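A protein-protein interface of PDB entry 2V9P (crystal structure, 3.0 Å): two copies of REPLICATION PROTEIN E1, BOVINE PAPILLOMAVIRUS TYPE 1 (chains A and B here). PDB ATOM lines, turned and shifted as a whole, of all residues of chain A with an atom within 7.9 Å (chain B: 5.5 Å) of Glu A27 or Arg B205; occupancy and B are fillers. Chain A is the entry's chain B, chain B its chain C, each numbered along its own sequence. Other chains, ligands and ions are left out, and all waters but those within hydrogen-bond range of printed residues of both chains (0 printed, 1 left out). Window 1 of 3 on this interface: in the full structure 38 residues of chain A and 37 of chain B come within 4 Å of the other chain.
NH2 of Arg A66 is in salt-bridge range of OE2 of Glu A28 (3.96 Å).
The guanidinium group (NH2) of Arg B70 sits at hydrogen-bond distance from the backbone carbonyl oxygen (O) of Ala B170 (2.8 Å).
The backbone NH of Ile B203 is in hydrogen-bond range of the backbone carbonyl oxygen of Val B211 (2.7 Å).
NH2 of Arg B205 lies within hydrogen-bond range of O of Ala B209.
Of the 23 printed residues of chain A, 4 touch a printed residue of chain B.
Position printed for both chains: 206.
Of the 9 pairs that touch across the chains among the printed residues, none has its exchanged pair printed and touching as well.
Among the printed residues, merely in contact across the chains: Lys A206 with Ala B209, Lys A206 with His B207, Glu A28 with Lys B208, Glu A27 with Val B211 and Lys A206 with Arg B205.
The guanidinium group (NH1) of Arg B70 lies within salt-bridge range of the side-chain carboxylate (OE2) of Glu A27.
OE1 of Glu A27 lies within salt-bridge range of NH1 of Arg B205.
OG of Ser A29 is in hydrogen-bond range of NH1 of Arg B70, 2.8 Å away.
The side-chain amino group of Lys A206 lies close to the backbone carbonyl oxygen of Lys B208 (2.4 Å).
Glu A27 touches just these residues of chain B: Arg B70, Arg B205 and Val B211.
Printed residues of chain B within 4 Å of Glu A28: Lys B208 (3.6 Å).
Thr A63 touches none of the printed residues of chain B.
Of the printed residues of chain B, Lys A206 touches Arg B205 (3.9 Å), His B207 (3.5 Å), Lys B208 (2.4 Å) and Ala B209 (3.5 Å).
Of the printed residues of chain A, Arg B70 touches Glu A27 and Ser A29.
Phe B164 touches none of the printed residues of chain A.
Of the printed residues of chain A, His B207 touches Lys A206.
The nearest residue of chain A that does not touch Arg B205 is Ser A29 (5.4 Å).
The nearest printed residue of chain B that does not touch Ser A29 is Arg B205 (5.4 Å).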
ATOM      1  N   TRP A  19       3.811   7.517  12.953  1.00  0.00           N
ATOM      2  CA  TRP A  19       3.094   8.698  13.400  1.00  0.00           C
ATOM      3  C   TRP A  19       1.999   8.296  14.371  1.00  0.00           C
ATOM      4  O   TRP A  19       1.989   8.752  15.517  1.00  0.00           O
ATOM      5  CB  TRP A  19       2.515   9.440  12.194  1.00  0.00           C
ATOM      6  CG  TRP A  19       1.572  10.544  12.544  1.00  0.00           C
ATOM      7  CD1 TRP A  19       1.900  11.826  12.869  1.00  0.00           C
ATOM      8  CD2 TRP A  19       0.137  10.468  12.599  1.00  0.00           C
ATOM      9  NE1 TRP A  19       0.767  12.556  13.128  1.00  0.00           N
ATOM     10  CE2 TRP A  19      -0.333  11.749  12.968  1.00  0.00           C
ATOM     11  CE3 TRP A  19      -0.798   9.443  12.370  1.00  0.00           C
ATOM     12  CZ2 TRP A  19      -1.704  12.038  13.113  1.00  0.00           C
ATOM     13  CZ3 TRP A  19      -2.152   9.728  12.517  1.00  0.00           C
ATOM     14  CH2 TRP A  19      -2.589  11.021  12.881  1.00  0.00           C
ATOM     15  N   ALA A  20       1.108   7.414  13.914  1.00  0.00           N
ATOM     16  CA  ALA A  20      -0.054   6.994  14.690  1.00  0.00           C
ATOM     17  C   ALA A  20       0.363   6.419  16.043  1.00  0.00           C
ATOM     18  O   ALA A  20      -0.193   6.779  17.095  1.00  0.00           O
ATOM     19  CB  ALA A  20      -0.886   5.997  13.895  1.00  0.00           C
ATOM     20  N   LYS A  24      -0.181   7.754  19.897  1.00  0.00           N
ATOM     21  CA  LYS A  24      -1.091   6.766  20.494  1.00  0.00           C
ATOM     22  C   LYS A  24      -2.500   6.808  19.900  1.00  0.00           C
ATOM     23  O   LYS A  24      -3.483   6.558  20.598  1.00  0.00           O
ATOM     24  CB  LYS A  24      -1.166   6.916  22.025  1.00  0.00           C
ATOM     25  CG  LYS A  24       0.175   6.992  22.746  1.00  0.00           C
ATOM     26  CD  LYS A  24       0.994   5.721  22.601  1.00  0.00           C
ATOM     27  CE  LYS A  24       2.413   5.930  23.092  1.00  0.00           C
ATOM     28  NZ  LYS A  24       3.375   5.109  22.312  1.00  0.00           N
ATOM     29  N   TYR A  25      -2.601   7.132  18.616  1.00  0.00           N
ATOM     30  CA  TYR A  25      -3.887   7.132  17.948  1.00  0.00           C
ATOM     31  C   TYR A  25      -4.209   5.719  17.462  1.00  0.00           C
ATOM     32  O   TYR A  25      -3.535   5.202  16.552  1.00  0.00           O
ATOM     33  CB  TYR A  25      -3.878   8.120  16.787  1.00  0.00           C
ATOM     34  CG  TYR A  25      -3.656   9.577  17.163  1.00  0.00           C
ATOM     35  CD1 TYR A  25      -3.048  10.451  16.256  1.00  0.00           C
ATOM     36  CD2 TYR A  25      -4.065  10.093  18.400  1.00  0.00           C
ATOM     37  CE1 TYR A  25      -2.850  11.790  16.561  1.00  0.00           C
ATOM     38  CE2 TYR A  25      -3.864  11.436  18.718  1.00  0.00           C
ATOM     39  CZ  TYR A  25      -3.254  12.274  17.785  1.00  0.00           C
ATOM     40  OH  TYR A  25      -3.038  13.601  18.051  1.00  0.00           O
ATOM     41  N   ALA A  26      -5.226   5.104  18.080  1.00  0.00           N
ATOM     42  CA  ALA A  26      -5.611   3.708  17.788  1.00  0.00           C
ATOM     43  C   ALA A  26      -6.930   3.590  17.035  1.00  0.00           C
ATOM     44  O   ALA A  26      -7.362   2.495  16.653  1.00  0.00           O
ATOM     45  CB  ALA A  26      -5.678   2.900  19.063  1.00  0.00           C
ATOM     46  N   GLU A  27      -7.553   4.727  16.797  1.00  0.00           N
ATOM     47  CA  GLU A  27      -8.897   4.736  16.331  1.00  0.00           C
ATOM     48  C   GLU A  27      -9.043   5.249  14.916  1.00  0.00           C
ATOM     49  O   GLU A  27      -8.695   6.388  14.629  1.00  0.00           O
ATOM     50  CB  GLU A  27      -9.695   5.585  17.281  1.00  0.00           C
ATOM     51  CG  GLU A  27     -10.667   4.805  18.048  1.00  0.00           C
ATOM     52  CD  GLU A  27     -12.052   5.046  17.493  1.00  0.00           C
ATOM     53  OE1 GLU A  27     -12.509   4.322  16.491  1.00  0.00           O
ATOM     54  OE2 GLU A  27     -12.685   6.009  18.062  1.00  0.00           O
ATOM     55  N   GLU A  28      -9.593   4.405  14.048  1.00  0.00           N
ATOM     56  CA  GLU A  28      -9.653   4.694  12.625  1.00  0.00           C
ATOM     57  C   GLU A  28     -10.032   6.136  12.329  1.00  0.00           C
ATOM     58  O   GLU A  28      -9.324   6.817  11.583  1.00  0.00           O
ATOM     59  CB  GLU A  28     -10.576   3.707  11.911  1.00  0.00           C
ATOM     60  CG  GLU A  28      -9.851   2.456  11.504  1.00  0.00           C
ATOM     61  CD  GLU A  28     -10.762   1.357  11.036  1.00  0.00           C
ATOM     62  OE1 GLU A  28     -11.875   1.652  10.548  1.00  0.00           O
ATOM     63  OE2 GLU A  28     -10.340   0.186  11.150  1.00  0.00           O
ATOM     64  N   SER A  29     -11.120   6.602  12.943  1.00  0.00           N
ATOM     65  CA  SER A  29     -11.648   7.946  12.666  1.00  0.00           C
ATOM     66  C   SER A  29     -10.656   9.016  13.055  1.00  0.00           C
ATOM     67  O   SER A  29     -10.300   9.876  12.245  1.00  0.00           O
ATOM     68  CB  SER A  29     -13.010   8.195  13.336  1.00  0.00           C
ATOM     69  OG  SER A  29     -12.996   7.827  14.697  1.00  0.00           O
ATOM     70  N   LYS A  30     -10.184   8.943  14.288  1.00  0.00           N
ATOM     71  CA  LYS A  30      -9.132   9.844  14.729  1.00  0.00           C
ATOM     72  C   LYS A  30      -7.850   9.790  13.881  1.00  0.00           C
ATOM     73  O   LYS A  30      -7.322  10.832  13.523  1.00  0.00           O
ATOM     74  CB  LYS A  30      -8.789   9.603  16.188  1.00  0.00           C
ATOM     75  CG  LYS A  30      -7.609  10.437  16.639  1.00  0.00           C
ATOM     76  CD  LYS A  30      -7.701  10.813  18.094  1.00  0.00           C
ATOM     77  CE  LYS A  30      -7.439  12.312  18.257  1.00  0.00           C
ATOM     78  NZ  LYS A  30      -7.114  12.635  19.668  1.00  0.00           N
ATOM     79  N   ILE A  31      -7.347   8.592  13.579  1.00  0.00           N
ATOM     80  CA  ILE A  31      -6.176   8.434  12.702  1.00  0.00           C
ATOM     81  C   ILE A  31      -6.385   9.128  11.354  1.00  0.00           C
ATOM     82  O   ILE A  31      -5.569   9.943  10.945  1.00  0.00           O
ATOM     83  CB  ILE A  31      -5.824   6.945  12.477  1.00  0.00           C
ATOM     84  CG1 ILE A  31      -5.373   6.311  13.795  1.00  0.00           C
ATOM     85  CG2 ILE A  31      -4.751   6.794  11.385  1.00  0.00           C
ATOM     86  CD1 ILE A  31      -5.199   4.806  13.756  1.00  0.00           C
ATOM     87  N   ALA A  32      -7.492   8.807  10.685  1.00  0.00           N
ATOM     88  CA  ALA A  32      -7.806   9.385   9.387  1.00  0.00           C
ATOM     89  C   ALA A  32      -7.793  10.899   9.481  1.00  0.00           C
ATOM     90  O   ALA A  32      -7.090  11.577   8.729  1.00  0.00           O
ATOM     91  CB  ALA A  32      -9.162   8.890   8.895  1.00  0.00           C
ATOM     92  N   TYR A  33      -8.550  11.419  10.436  1.00  0.00           N
ATOM     93  CA  TYR A  33      -8.803  12.847  10.514  1.00  0.00           C
ATOM     94  C   TYR A  33      -7.584  13.633  10.897  1.00  0.00           C
ATOM     95  O   TYR A  33      -7.299  14.685  10.343  1.00  0.00           O
ATOM     96  CB  TYR A  33      -9.898  13.126  11.533  1.00  0.00           C
ATOM     97  CG  TYR A  33     -10.160  14.601  11.758  1.00  0.00           C
ATOM     98  CD1 TYR A  33     -10.676  15.405  10.738  1.00  0.00           C
ATOM     99  CD2 TYR A  33      -9.909  15.188  12.995  1.00  0.00           C
ATOM    100  CE1 TYR A  33     -10.926  16.760  10.949  1.00  0.00           C
ATOM    101  CE2 TYR A  33     -10.160  16.532  13.216  1.00  0.00           C
ATOM    102  CZ  TYR A  33     -10.662  17.314  12.193  1.00  0.00           C
ATOM    103  OH  TYR A  33     -10.900  18.649  12.411  1.00  0.00           O
ATOM    104  N   GLU A  34      -6.873  13.102  11.870  1.00  0.00           N
ATOM    105  CA  GLU A  34      -5.748  13.774  12.468  1.00  0.00           C
ATOM    106  C   GLU A  34      -4.552  13.791  11.527  1.00  0.00           C
ATOM    107  O   GLU A  34      -3.746  14.714  11.561  1.00  0.00           O
ATOM    108  CB  GLU A  34      -5.396  13.077  13.783  1.00  0.00           C
ATOM    109  CG  GLU A  34      -4.672  13.951  14.786  1.00  0.00           C
ATOM    110  CD  GLU A  34      -5.475  15.163  15.227  1.00  0.00           C
ATOM    111  OE1 GLU A  34      -6.568  14.971  15.789  1.00  0.00           O
ATOM    112  OE2 GLU A  34      -5.004  16.304  15.027  1.00  0.00           O
ATOM    113  N   VAL A  58      -6.161   3.650   6.425  1.00  0.00           N
ATOM    114  CA  VAL A  58      -6.650   4.033   7.737  1.00  0.00           C
ATOM    115  C   VAL A  58      -6.994   2.794   8.561  1.00  0.00           C
ATOM    116  O   VAL A  58      -6.646   2.696   9.740  1.00  0.00           O
ATOM    117  CB  VAL A  58      -7.879   4.935   7.602  1.00  0.00           C
ATOM    118  CG1 VAL A  58      -8.477   5.243   8.953  1.00  0.00           C
ATOM    119  CG2 VAL A  58      -7.493   6.213   6.894  1.00  0.00           C
ATOM    120  N   LYS A  59      -7.676   1.849   7.921  1.00  0.00           N
ATOM    121  CA  LYS A  59      -8.068   0.609   8.562  1.00  0.00           C
ATOM    122  C   LYS A  59      -6.836  -0.179   8.999  1.00  0.00           C
ATOM    123  O   LYS A  59      -6.708  -0.496  10.175  1.00  0.00           O
ATOM    124  CB  LYS A  59      -8.930  -0.197   7.615  1.00  0.00           C
ATOM    125  CG  LYS A  59      -9.604  -1.393   8.217  1.00  0.00           C
ATOM    126  CD  LYS A  59     -10.276  -2.158   7.085  1.00  0.00           C
ATOM    127  CE  LYS A  59     -11.121  -3.297   7.585  1.00  0.00           C
ATOM    128  NZ  LYS A  59     -10.236  -4.443   7.938  1.00  0.00           N
ATOM    129  N   CYS A  61      -3.814   0.815   9.385  1.00  0.00           N
ATOM    130  CA  CYS A  61      -3.039   1.574  10.360  1.00  0.00           C
ATOM    131  C   CYS A  61      -3.534   1.293  11.772  1.00  0.00           C
ATOM    132  O   CYS A  61      -2.752   0.949  12.659  1.00  0.00           O
ATOM    133  CB  CYS A  61      -3.076   3.079  10.077  1.00  0.00           C
ATOM    134  SG  CYS A  61      -2.022   4.052  11.213  1.00  0.00           S
ATOM    135  N   ALA A  62      -4.839   1.430  11.974  1.00  0.00           N
ATOM    136  CA  ALA A  62      -5.429   1.139  13.266  1.00  0.00           C
ATOM    137  C   ALA A  62      -5.100  -0.296  13.687  1.00  0.00           C
ATOM    138  O   ALA A  62      -4.654  -0.512  14.812  1.00  0.00           O
ATOM    139  CB  ALA A  62      -6.921   1.379  13.235  1.00  0.00           C
ATOM    140  N   THR A  63      -5.286  -1.264  12.783  1.00  0.00           N
ATOM    141  CA  THR A  63      -4.935  -2.657  13.062  1.00  0.00           C
ATOM    142  C   THR A  63      -3.513  -2.729  13.582  1.00  0.00           C
ATOM    143  O   THR A  63      -3.243  -3.335  14.618  1.00  0.00           O
ATOM    144  CB  THR A  63      -4.981  -3.526  11.812  1.00  0.00           C
ATOM    145  OG1 THR A  63      -6.145  -3.211  11.048  1.00  0.00           O
ATOM    146  CG2 THR A  63      -5.004  -4.986  12.190  1.00  0.00           C
ATOM    147  N   VAL A  65      -1.389  -0.362  14.752  1.00  0.00           N
ATOM    148  CA  VAL A  65      -1.133   0.294  16.024  1.00  0.00           C
ATOM    149  C   VAL A  65      -1.676  -0.566  17.152  1.00  0.00           C
ATOM    150  O   VAL A  65      -0.959  -0.833  18.115  1.00  0.00           O
ATOM    151  CB  VAL A  65      -1.729   1.700  16.079  1.00  0.00           C
ATOM    152  CG1 VAL A  65      -1.503   2.324  17.434  1.00  0.00           C
ATOM    153  CG2 VAL A  65      -1.106   2.566  15.009  1.00  0.00           C
ATOM    154  N   ARG A  66      -2.924  -1.024  17.013  1.00  0.00           N
ATOM    155  CA  ARG A  66      -3.534  -1.945  17.977  1.00  0.00           C
ATOM    156  C   ARG A  66      -2.618  -3.132  18.271  1.00  0.00           C
ATOM    157  O   ARG A  66      -2.424  -3.479  19.430  1.00  0.00           O
ATOM    158  CB  ARG A  66      -4.916  -2.412  17.505  1.00  0.00           C
ATOM    159  CG  ARG A  66      -6.032  -1.420  17.787  1.00  0.00           C
ATOM    160  CD  ARG A  66      -7.435  -1.970  17.499  1.00  0.00           C
ATOM    161  NE  ARG A  66      -7.934  -1.568  16.175  1.00  0.00           N
ATOM    162  CZ  ARG A  66      -7.970  -2.358  15.095  1.00  0.00           C
ATOM    163  NH1 ARG A  66      -7.549  -3.623  15.156  1.00  0.00           N
ATOM    164  NH2 ARG A  66      -8.430  -1.882  13.936  1.00  0.00           N
ATOM    165  N   LEU A  69       0.500  -1.736  20.326  1.00  0.00           N
ATOM    166  CA  LEU A  69       0.095  -1.306  21.665  1.00  0.00           C
ATOM    167  C   LEU A  69      -0.230  -2.501  22.550  1.00  0.00           C
ATOM    168  O   LEU A  69       0.281  -2.597  23.676  1.00  0.00           O
ATOM    169  CB  LEU A  69      -1.104  -0.352  21.606  1.00  0.00           C
ATOM    170  CG  LEU A  69      -0.873   1.055  21.073  1.00  0.00           C
ATOM    171  CD1 LEU A  69      -2.168   1.844  21.178  1.00  0.00           C
ATOM    172  CD2 LEU A  69       0.233   1.727  21.838  1.00  0.00           C
ATOM    173  N   ASN A 159     -24.017  -5.442  26.888  1.00  0.00           N
ATOM    174  CA  ASN A 159     -23.664  -6.153  25.654  1.00  0.00           C
ATOM    175  C   ASN A 159     -23.419  -7.655  25.832  1.00  0.00           C
ATOM    176  O   ASN A 159     -22.878  -8.309  24.929  1.00  0.00           O
ATOM    177  CB  ASN A 159     -22.418  -5.525  25.010  1.00  0.00           C
ATOM    178  CG  ASN A 159     -22.570  -4.053  24.785  1.00  0.00           C
ATOM    179  OD1 ASN A 159     -23.617  -3.588  24.334  1.00  0.00           O
ATOM    180  ND2 ASN A 159     -21.535  -3.297  25.111  1.00  0.00           N
ATOM    181  N   LYS A 206     -12.745 -10.039  17.419  1.00  0.00           N
ATOM    182  CA  LYS A 206     -13.525  -9.790  16.208  1.00  0.00           C
ATOM    183  C   LYS A 206     -12.961 -10.393  14.925  1.00  0.00           C
ATOM    184  O   LYS A 206     -13.543 -11.314  14.338  1.00  0.00           O
ATOM    185  CB  LYS A 206     -13.764  -8.292  16.024  1.00  0.00           C
ATOM    186  CG  LYS A 206     -14.959  -7.774  16.796  1.00  0.00           C
ATOM    187  CD  LYS A 206     -16.240  -7.874  15.984  1.00  0.00           C
ATOM    188  CE  LYS A 206     -16.463  -6.625  15.143  1.00  0.00           C
ATOM    189  NZ  LYS A 206     -16.612  -5.407  15.994  1.00  0.00           N
ATOM    190  N   ARG B  70     -16.940  12.605  12.749  1.00  0.00           N
ATOM    191  CA  ARG B  70     -16.869  12.113  14.111  1.00  0.00           C
ATOM    192  C   ARG B  70     -15.696  12.763  14.821  1.00  0.00           C
ATOM    193  O   ARG B  70     -15.849  13.363  15.884  1.00  0.00           O
ATOM    194  CB  ARG B  70     -16.690  10.601  14.122  1.00  0.00           C
ATOM    195  CG  ARG B  70     -16.616  10.034  15.510  1.00  0.00           C
ATOM    196  CD  ARG B  70     -16.500   8.530  15.513  1.00  0.00           C
ATOM    197  NE  ARG B  70     -16.555   8.066  16.890  1.00  0.00           N
ATOM    198  CZ  ARG B  70     -15.488   7.866  17.658  1.00  0.00           C
ATOM    199  NH1 ARG B  70     -14.258   8.054  17.169  1.00  0.00           N
ATOM    200  NH2 ARG B  70     -15.655   7.466  18.913  1.00  0.00           N
ATOM    201  N   PHE B 164     -25.851  -3.233  18.474  1.00  0.00           N
ATOM    202  CA  PHE B 164     -25.398  -1.954  17.978  1.00  0.00           C
ATOM    203  C   PHE B 164     -26.385  -0.815  18.201  1.00  0.00           C
ATOM    204  O   PHE B 164     -26.199   0.277  17.663  1.00  0.00           O
ATOM    205  CB  PHE B 164     -25.003  -2.095  16.504  1.00  0.00           C
ATOM    206  CG  PHE B 164     -24.149  -3.298  16.235  1.00  0.00           C
ATOM    207  CD1 PHE B 164     -22.803  -3.298  16.590  1.00  0.00           C
ATOM    208  CD2 PHE B 164     -24.691  -4.448  15.660  1.00  0.00           C
ATOM    209  CE1 PHE B 164     -22.004  -4.414  16.359  1.00  0.00           C
ATOM    210  CE2 PHE B 164     -23.904  -5.563  15.430  1.00  0.00           C
ATOM    211  CZ  PHE B 164     -22.557  -5.542  15.779  1.00  0.00           C
ATOM    212  N   ALA B 167     -24.832   2.328  19.347  1.00  0.00           N
ATOM    213  CA  ALA B 167     -23.629   2.666  18.596  1.00  0.00           C
ATOM    214  C   ALA B 167     -23.414   4.171  18.403  1.00  0.00           C
ATOM    215  O   ALA B 167     -22.282   4.610  18.201  1.00  0.00           O
ATOM    216  CB  ALA B 167     -23.623   1.947  17.262  1.00  0.00           C
ATOM    217  N   ALA B 170     -21.105   6.488  20.640  1.00  0.00           N
ATOM    218  CA  ALA B 170     -19.697   6.650  20.334  1.00  0.00           C
ATOM    219  C   ALA B 170     -19.449   7.918  19.524  1.00  0.00           C
ATOM    220  O   ALA B 170     -18.296   8.315  19.362  1.00  0.00           O
ATOM    221  CB  ALA B 170     -19.169   5.438  19.612  1.00  0.00           C
ATOM    222  N   ILE B 203     -18.776   0.538  23.891  1.00  0.00           N
ATOM    223  CA  ILE B 203     -19.806   0.697  22.880  1.00  0.00           C
ATOM    224  C   ILE B 203     -19.448  -0.099  21.651  1.00  0.00           C
ATOM    225  O   ILE B 203     -18.397   0.085  21.050  1.00  0.00           O
ATOM    226  CB  ILE B 203     -19.998   2.176  22.488  1.00  0.00           C
ATOM    227  CG1 ILE B 203     -20.518   2.994  23.679  1.00  0.00           C
ATOM    228  CG2 ILE B 203     -20.907   2.295  21.265  1.00  0.00           C
ATOM    229  CD1 ILE B 203     -21.988   2.758  24.033  1.00  0.00           C
ATOM    230  N   ASP B 204     -20.357  -0.977  21.280  1.00  0.00           N
ATOM    231  CA  ASP B 204     -20.151  -1.891  20.182  1.00  0.00           C
ATOM    232  C   ASP B 204     -20.511  -1.206  18.853  1.00  0.00           C
ATOM    233  O   ASP B 204     -21.654  -0.790  18.646  1.00  0.00           O
ATOM    234  CB  ASP B 204     -21.028  -3.116  20.434  1.00  0.00           C
ATOM    235  CG  ASP B 204     -20.445  -4.376  19.884  1.00  0.00           C
ATOM    236  OD1 ASP B 204     -19.672  -4.282  18.906  1.00  0.00           O
ATOM    237  OD2 ASP B 204     -20.782  -5.462  20.424  1.00  0.00           O
ATOM    238  N   ARG B 205     -19.528  -1.059  17.971  1.00  0.00           N
ATOM    239  CA  ARG B 205     -19.787  -0.505  16.653  1.00  0.00           C
ATOM    240  C   ARG B 205     -19.922  -1.635  15.677  1.00  0.00           C
ATOM    241  O   ARG B 205     -19.353  -2.699  15.894  1.00  0.00           O
ATOM    242  CB  ARG B 205     -18.676   0.428  16.202  1.00  0.00           C
ATOM    243  CG  ARG B 205     -18.817   1.870  16.672  1.00  0.00           C
ATOM    244  CD  ARG B 205     -17.820   2.144  17.762  1.00  0.00           C
ATOM    245  NE  ARG B 205     -16.510   1.577  17.439  1.00  0.00           N
ATOM    246  CZ  ARG B 205     -15.516   2.250  16.867  1.00  0.00           C
ATOM    247  NH1 ARG B 205     -15.658   3.539  16.559  1.00  0.00           N
ATOM    248  NH2 ARG B 205     -14.369   1.632  16.617  1.00  0.00           N
ATOM    249  N   LYS B 206     -20.658  -1.387  14.592  1.00  0.00           N
ATOM    250  CA  LYS B 206     -21.092  -2.451  13.688  1.00  0.00           C
ATOM    251  C   LYS B 206     -19.954  -3.250  13.082  1.00  0.00           C
ATOM    252  O   LYS B 206     -19.818  -4.443  13.380  1.00  0.00           O
ATOM    253  CB  LYS B 206     -22.083  -1.969  12.622  1.00  0.00           C
ATOM    254  CG  LYS B 206     -23.073  -3.073  12.238  1.00  0.00           C
ATOM    255  CD  LYS B 206     -24.319  -2.565  11.531  1.00  0.00           C
ATOM    256  CE  LYS B 206     -25.271  -3.730  11.233  1.00  0.00           C
ATOM    257  NZ  LYS B 206     -26.597  -3.237  10.793  1.00  0.00           N
ATOM    258  N   HIS B 207     -19.134  -2.649  12.232  1.00  0.00           N
ATOM    259  CA  HIS B 207     -18.065  -3.490  11.726  1.00  0.00           C
ATOM    260  C   HIS B 207     -16.686  -3.294  12.368  1.00  0.00           C
ATOM    261  O   HIS B 207     -15.947  -4.275  12.557  1.00  0.00           O
ATOM    262  CB  HIS B 207     -18.114  -3.725  10.200  1.00  0.00           C
ATOM    263  CG  HIS B 207     -18.556  -5.123   9.842  1.00  0.00           C
ATOM    264  ND1 HIS B 207     -17.720  -6.044   9.237  1.00  0.00           N
ATOM    265  CD2 HIS B 207     -19.724  -5.777  10.078  1.00  0.00           C
ATOM    266  CE1 HIS B 207     -18.365  -7.189   9.082  1.00  0.00           C
ATOM    267  NE2 HIS B 207     -19.581  -7.054   9.586  1.00  0.00           N
ATOM    268  N   LYS B 208     -16.386  -2.054  12.763  1.00  0.00           N
ATOM    269  CA  LYS B 208     -15.265  -1.765  13.675  1.00  0.00           C
ATOM    270  C   LYS B 208     -15.360  -2.534  15.013  1.00  0.00           C
ATOM    271  O   LYS B 208     -16.371  -3.165  15.305  1.00  0.00           O
ATOM    272  CB  LYS B 208     -15.171  -0.259  13.936  1.00  0.00           C
ATOM    273  CG  LYS B 208     -14.381   0.495  12.871  1.00  0.00           C
ATOM    274  CD  LYS B 208     -14.330   2.015  13.151  1.00  0.00           C
ATOM    275  CE  LYS B 208     -15.322   2.831  12.295  1.00  0.00           C
ATOM    276  NZ  LYS B 208     -16.757   2.600  12.652  1.00  0.00           N
ATOM    277  N   ALA B 209     -14.295  -2.488  15.809  1.00  0.00           N
ATOM    278  CA  ALA B 209     -14.296  -3.090  17.147  1.00  0.00           C
ATOM    279  C   ALA B 209     -14.829  -2.078  18.130  1.00  0.00           C
ATOM    280  O   ALA B 209     -14.835  -0.874  17.844  1.00  0.00           O
ATOM    281  CB  ALA B 209     -12.897  -3.522  17.551  1.00  0.00           C
ATOM    282  N   ALA B 210     -15.262  -2.566  19.287  1.00  0.00           N
ATOM    283  CA  ALA B 210     -15.857  -1.723  20.317  1.00  0.00           C
ATOM    284  C   ALA B 210     -14.969  -0.522  20.700  1.00  0.00           C
ATOM    285  O   ALA B 210     -13.751  -0.587  20.547  1.00  0.00           O
ATOM    286  CB  ALA B 210     -16.161  -2.563  21.536  1.00  0.00           C
ATOM    287  N   VAL B 211     -15.563   0.579  21.167  1.00  0.00           N
ATOM    288  CA  VAL B 211     -14.773   1.600  21.867  1.00  0.00           C
ATOM    289  C   VAL B 211     -15.258   1.875  23.267  1.00  0.00           C
ATOM    290  O   VAL B 211     -16.458   1.916  23.529  1.00  0.00           O
ATOM    291  CB  VAL B 211     -14.659   2.960  21.144  1.00  0.00           C
ATOM    292  CG1 VAL B 211     -13.570   2.903  20.077  1.00  0.00           C
ATOM    293  CG2 VAL B 211     -16.006   3.432  20.615  1.00  0.00           C
